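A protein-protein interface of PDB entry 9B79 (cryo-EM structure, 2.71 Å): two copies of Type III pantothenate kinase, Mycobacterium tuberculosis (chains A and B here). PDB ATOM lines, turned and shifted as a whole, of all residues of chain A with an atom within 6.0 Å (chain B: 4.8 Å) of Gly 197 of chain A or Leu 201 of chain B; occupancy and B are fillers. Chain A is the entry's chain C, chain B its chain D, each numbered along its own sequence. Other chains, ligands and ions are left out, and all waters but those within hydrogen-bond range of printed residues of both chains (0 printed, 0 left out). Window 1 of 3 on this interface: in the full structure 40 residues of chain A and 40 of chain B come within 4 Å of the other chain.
O of Gly 200 of chain A sits close to O of Gly 200 of chain B, 3.1 Å away.
Among the printed residues, merely in contact across the chains: Phe 196 of chain A with Leu 205 of chain B, Gly 197 of chain A with Leu 201 of chain B, Gly 197 of chain A with Leu 205 of chain B, Leu 201 of chain A with Gly 197 of chain B, Leu 201 of chain A with Gly 200 of chain B and Leu 201 of chain A with Leu 201 of chain B.
Gly 197 of chain A touches two residues of chain B.
Printed residues of chain A within 4 Å of Leu 201 of chain B: Gly 197 and Leu 201.
Of the printed residues of chain B, Gly 200 of chain A touches Gly 200 (3.1 Å).
Of the printed residues of chain A, Gly 200 of chain B touches Gly 200 and Leu 201.
Of the printed residues of chain B, Phe 196 of chain A touches Leu 205 (3.8 Å).
Hydrophobic or aromatic side chains of chain B that line the printed part of chain A: Leu 201 and Leu 205.
Of the 11 printed residues of chain A, 4 touch a printed residue of chain B.
Hydrophobic or aromatic side chains of chain A that line the printed part of chain B: Phe 196 and Leu 201.
Among the printed residues, no Asp or Glu carboxylate lies within 4 Å of a Lys or Arg side-chain nitrogen of the other chain.
Gly 197 of chain A touches Leu 201 of chain B, and with the chains exchanged Leu 201 of chain A touches Gly 197 of chain B.
Gly 200 of chain A touches its own counterpart, Gly 200 of chain B.
Leu 201 of chain A touches Gly 200 of chain B, but with the chains exchanged Gly 200 of chain A does not touch Leu 201 of chain B (4.04 Å).
Leu 201 of chain A touches its own counterpart, Leu 201 of chain B.
6 positions are printed for both chains.
Of the 7 pairs that touch across the chains among the printed residues, 4 have their exchanged pair printed and touching as well.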
ATOM      1  N   ALA A 192     -20.728 -18.315  -9.601  1.00  0.00           N
ATOM      2  CA  ALA A 192     -21.803 -17.714 -10.379  1.00  0.00           C
ATOM      3  C   ALA A 192     -22.794 -18.764 -10.845  1.00  0.00           C
ATOM      4  O   ALA A 192     -24.008 -18.566 -10.740  1.00  0.00           O
ATOM      5  CB  ALA A 192     -21.224 -16.956 -11.570  1.00  0.00           C
ATOM      6  N   GLY A 193     -22.293 -19.900 -11.324  1.00  0.00           N
ATOM      7  CA  GLY A 193     -23.138 -21.025 -11.654  1.00  0.00           C
ATOM      8  C   GLY A 193     -24.012 -21.431 -10.491  1.00  0.00           C
ATOM      9  O   GLY A 193     -25.231 -21.277 -10.562  1.00  0.00           O
ATOM     10  N   ALA A 194     -23.394 -21.842  -9.381  1.00  0.00           N
ATOM     11  CA  ALA A 194     -24.147 -22.388  -8.256  1.00  0.00           C
ATOM     12  C   ALA A 194     -25.156 -21.387  -7.702  1.00  0.00           C
ATOM     13  O   ALA A 194     -26.257 -21.772  -7.295  1.00  0.00           O
ATOM     14  CB  ALA A 194     -23.188 -22.841  -7.158  1.00  0.00           C
ATOM     15  N   VAL A 195     -24.813 -20.101  -7.675  1.00  0.00           N
ATOM     16  CA  VAL A 195     -25.682 -19.126  -7.030  1.00  0.00           C
ATOM     17  C   VAL A 195     -26.747 -18.615  -7.994  1.00  0.00           C
ATOM     18  O   VAL A 195     -27.947 -18.798  -7.754  1.00  0.00           O
ATOM     19  CB  VAL A 195     -24.860 -17.962  -6.449  1.00  0.00           C
ATOM     20  CG1 VAL A 195     -25.773 -16.833  -5.998  1.00  0.00           C
ATOM     21  CG2 VAL A 195     -24.022 -18.456  -5.288  1.00  0.00           C
ATOM     22  N   PHE A 196     -26.324 -17.979  -9.091  1.00  0.00           N
ATOM     23  CA  PHE A 196     -27.291 -17.384 -10.004  1.00  0.00           C
ATOM     24  C   PHE A 196     -28.098 -18.442 -10.749  1.00  0.00           C
ATOM     25  O   PHE A 196     -29.293 -18.245 -10.994  1.00  0.00           O
ATOM     26  CB  PHE A 196     -26.577 -16.460 -10.989  1.00  0.00           C
ATOM     27  CG  PHE A 196     -25.944 -15.261 -10.343  1.00  0.00           C
ATOM     28  CD1 PHE A 196     -26.722 -14.278  -9.762  1.00  0.00           C
ATOM     29  CD2 PHE A 196     -24.568 -15.116 -10.322  1.00  0.00           C
ATOM     30  CE1 PHE A 196     -26.142 -13.175  -9.171  1.00  0.00           C
ATOM     31  CE2 PHE A 196     -23.982 -14.015  -9.732  1.00  0.00           C
ATOM     32  CZ  PHE A 196     -24.772 -13.043  -9.156  1.00  0.00           C
ATOM     33  N   GLY A 197     -27.474 -19.561 -11.132  1.00  0.00           N
ATOM     34  CA  GLY A 197     -28.218 -20.608 -11.799  1.00  0.00           C
ATOM     35  C   GLY A 197     -29.291 -21.217 -10.920  1.00  0.00           C
ATOM     36  O   GLY A 197     -30.393 -21.497 -11.383  1.00  0.00           O
ATOM     37  N   PHE A 198     -28.994 -21.416  -9.637  1.00  0.00           N
ATOM     38  CA  PHE A 198     -30.014 -21.989  -8.765  1.00  0.00           C
ATOM     39  C   PHE A 198     -31.068 -20.963  -8.362  1.00  0.00           C
ATOM     40  O   PHE A 198     -32.231 -21.330  -8.146  1.00  0.00           O
ATOM     41  CB  PHE A 198     -29.361 -22.619  -7.537  1.00  0.00           C
ATOM     42  CG  PHE A 198     -28.973 -24.055  -7.738  1.00  0.00           C
ATOM     43  CD1 PHE A 198     -29.909 -25.062  -7.604  1.00  0.00           C
ATOM     44  CD2 PHE A 198     -27.679 -24.397  -8.082  1.00  0.00           C
ATOM     45  CE1 PHE A 198     -29.557 -26.379  -7.796  1.00  0.00           C
ATOM     46  CE2 PHE A 198     -27.322 -25.714  -8.274  1.00  0.00           C
ATOM     47  CZ  PHE A 198     -28.263 -26.705  -8.132  1.00  0.00           C
ATOM     48  N   ALA A 199     -30.703 -19.680  -8.301  1.00  0.00           N
ATOM     49  CA  ALA A 199     -31.716 -18.640  -8.167  1.00  0.00           C
ATOM     50  C   ALA A 199     -32.667 -18.657  -9.358  1.00  0.00           C
ATOM     51  O   ALA A 199     -33.893 -18.599  -9.195  1.00  0.00           O
ATOM     52  CB  ALA A 199     -31.051 -17.272  -8.028  1.00  0.00           C
ATOM     53  N   GLY A 200     -32.114 -18.756 -10.569  1.00  0.00           N
ATOM     54  CA  GLY A 200     -32.946 -18.885 -11.750  1.00  0.00           C
ATOM     55  C   GLY A 200     -33.753 -20.165 -11.761  1.00  0.00           C
ATOM     56  O   GLY A 200     -34.871 -20.188 -12.269  1.00  0.00           O
ATOM     57  N   LEU A 201     -33.195 -21.245 -11.216  1.00  0.00           N
ATOM     58  CA  LEU A 201     -33.911 -22.512 -11.123  1.00  0.00           C
ATOM     59  C   LEU A 201     -35.160 -22.371 -10.266  1.00  0.00           C
ATOM     60  O   LEU A 201     -36.252 -22.810 -10.650  1.00  0.00           O
ATOM     61  CB  LEU A 201     -32.968 -23.576 -10.548  1.00  0.00           C
ATOM     62  CG  LEU A 201     -33.398 -25.005 -10.204  1.00  0.00           C
ATOM     63  CD1 LEU A 201     -32.203 -25.929 -10.323  1.00  0.00           C
ATOM     64  CD2 LEU A 201     -33.981 -25.115  -8.808  1.00  0.00           C
ATOM     65  N   VAL A 202     -35.010 -21.756  -9.091  1.00  0.00           N
ATOM     66  CA  VAL A 202     -36.154 -21.558  -8.207  1.00  0.00           C
ATOM     67  C   VAL A 202     -37.159 -20.596  -8.830  1.00  0.00           C
ATOM     68  O   VAL A 202     -38.376 -20.813  -8.752  1.00  0.00           O
ATOM     69  CB  VAL A 202     -35.678 -21.076  -6.825  1.00  0.00           C
ATOM     70  CG1 VAL A 202     -36.860 -20.857  -5.904  1.00  0.00           C
ATOM     71  CG2 VAL A 202     -34.726 -22.087  -6.222  1.00  0.00           C
ATOM     72  N   ILE B 136     -22.999 -27.936 -16.855  1.00  0.00           N
ATOM     73  CA  ILE B 136     -23.618 -27.015 -17.797  1.00  0.00           C
ATOM     74  C   ILE B 136     -22.724 -25.786 -17.875  1.00  0.00           C
ATOM     75  O   ILE B 136     -22.665 -24.986 -16.939  1.00  0.00           O
ATOM     76  CB  ILE B 136     -25.046 -26.649 -17.378  1.00  0.00           C
ATOM     77  CG1 ILE B 136     -25.943 -27.883 -17.431  1.00  0.00           C
ATOM     78  CG2 ILE B 136     -25.598 -25.551 -18.269  1.00  0.00           C
ATOM     79  CD1 ILE B 136     -27.358 -27.624 -16.995  1.00  0.00           C
ATOM     80  N   ALA B 153     -22.288 -24.314 -14.147  1.00  0.00           N
ATOM     81  CA  ALA B 153     -23.282 -24.880 -13.259  1.00  0.00           C
ATOM     82  C   ALA B 153     -23.143 -26.392 -13.222  1.00  0.00           C
ATOM     83  O   ALA B 153     -22.582 -26.995 -14.140  1.00  0.00           O
ATOM     84  CB  ALA B 153     -24.681 -24.488 -13.725  1.00  0.00           C
ATOM     85  N   GLY B 197     -36.504 -27.297 -13.400  1.00  0.00           N
ATOM     86  CA  GLY B 197     -35.559 -26.489 -12.663  1.00  0.00           C
ATOM     87  C   GLY B 197     -34.274 -26.219 -13.418  1.00  0.00           C
ATOM     88  O   GLY B 197     -33.755 -25.107 -13.368  1.00  0.00           O
ATOM     89  N   PHE B 198     -33.728 -27.214 -14.128  1.00  0.00           N
ATOM     90  CA  PHE B 198     -32.504 -26.918 -14.860  1.00  0.00           C
ATOM     91  C   PHE B 198     -32.772 -26.098 -16.117  1.00  0.00           C
ATOM     92  O   PHE B 198     -31.917 -25.301 -16.524  1.00  0.00           O
ATOM     93  CB  PHE B 198     -31.762 -28.211 -15.186  1.00  0.00           C
ATOM     94  CG  PHE B 198     -30.753 -28.592 -14.142  1.00  0.00           C
ATOM     95  CD1 PHE B 198     -29.518 -27.975 -14.097  1.00  0.00           C
ATOM     96  CD2 PHE B 198     -31.049 -29.553 -13.190  1.00  0.00           C
ATOM     97  CE1 PHE B 198     -28.597 -28.313 -13.132  1.00  0.00           C
ATOM     98  CE2 PHE B 198     -30.128 -29.898 -12.223  1.00  0.00           C
ATOM     99  CZ  PHE B 198     -28.900 -29.278 -12.195  1.00  0.00           C
ATOM    100  N   ALA B 199     -33.958 -26.239 -16.716  1.00  0.00           N
ATOM    101  CA  ALA B 199     -34.363 -25.297 -17.753  1.00  0.00           C
ATOM    102  C   ALA B 199     -34.449 -23.878 -17.203  1.00  0.00           C
ATOM    103  O   ALA B 199     -33.992 -22.925 -17.845  1.00  0.00           O
ATOM    104  CB  ALA B 199     -35.700 -25.722 -18.356  1.00  0.00           C
ATOM    105  N   GLY B 200     -35.014 -23.723 -16.004  1.00  0.00           N
ATOM    106  CA  GLY B 200     -35.041 -22.421 -15.365  1.00  0.00           C
ATOM    107  C   GLY B 200     -33.667 -21.922 -14.976  1.00  0.00           C
ATOM    108  O   GLY B 200     -33.422 -20.719 -14.984  1.00  0.00           O
ATOM    109  N   LEU B 201     -32.761 -22.835 -14.627  1.00  0.00           N
ATOM    110  CA  LEU B 201     -31.375 -22.476 -14.347  1.00  0.00           C
ATOM    111  C   LEU B 201     -30.714 -21.870 -15.574  1.00  0.00           C
ATOM    112  O   LEU B 201     -30.092 -20.802 -15.500  1.00  0.00           O
ATOM    113  CB  LEU B 201     -30.618 -23.722 -13.873  1.00  0.00           C
ATOM    114  CG  LEU B 201     -29.137 -23.698 -13.474  1.00  0.00           C
ATOM    115  CD1 LEU B 201     -28.872 -24.762 -12.425  1.00  0.00           C
ATOM    116  CD2 LEU B 201     -28.218 -23.919 -14.662  1.00  0.00           C
ATOM    117  N   VAL B 202     -30.855 -22.538 -16.721  1.00  0.00           N
ATOM    118  CA  VAL B 202     -30.294 -22.020 -17.965  1.00  0.00           C
ATOM    119  C   VAL B 202     -30.936 -20.687 -18.330  1.00  0.00           C
ATOM    120  O   VAL B 202     -30.243 -19.726 -18.691  1.00  0.00           O
ATOM    121  CB  VAL B 202     -30.452 -23.056 -19.093  1.00  0.00           C
ATOM    122  CG1 VAL B 202     -29.931 -22.499 -20.405  1.00  0.00           C
ATOM    123  CG2 VAL B 202     -29.725 -24.340 -18.737  1.00  0.00           C
ATOM    124  N   ASP B 203     -32.265 -20.597 -18.217  1.00  0.00           N
ATOM    125  CA  ASP B 203     -32.958 -19.361 -18.565  1.00  0.00           C
ATOM    126  C   ASP B 203     -32.567 -18.215 -17.640  1.00  0.00           C
ATOM    127  O   ASP B 203     -32.377 -17.084 -18.094  1.00  0.00           O
ATOM    128  CB  ASP B 203     -34.469 -19.581 -18.529  1.00  0.00           C
ATOM    129  CG  ASP B 203     -34.982 -20.291 -19.762  1.00  0.00           C
ATOM    130  OD1 ASP B 203     -34.432 -20.055 -20.857  1.00  0.00           O
ATOM    131  OD2 ASP B 203     -35.936 -21.087 -19.637  1.00  0.00           O
ATOM    132  N   GLY B 204     -32.442 -18.487 -16.342  1.00  0.00           N
ATOM    133  CA  GLY B 204     -32.057 -17.450 -15.405  1.00  0.00           C
ATOM    134  C   GLY B 204     -30.632 -16.979 -15.609  1.00  0.00           C
ATOM    135  O   GLY B 204     -30.358 -15.780 -15.549  1.00  0.00           O
ATOM    136  N   LEU B 205     -29.711 -17.911 -15.873  1.00  0.00           N
ATOM    137  CA  LEU B 205     -28.338 -17.520 -16.184  1.00  0.00           C
ATOM    138  C   LEU B 205     -28.283 -16.658 -17.438  1.00  0.00           C
ATOM    139  O   LEU B 205     -27.621 -15.613 -17.456  1.00  0.00           O
ATOM    140  CB  LEU B 205     -27.462 -18.762 -16.344  1.00  0.00           C
ATOM    141  CG  LEU B 205     -26.862 -19.332 -15.059  1.00  0.00           C
ATOM    142  CD1 LEU B 205     -25.972 -20.523 -15.362  1.00  0.00           C
ATOM    143  CD2 LEU B 205     -26.089 -18.258 -14.313  1.00  0.00           C
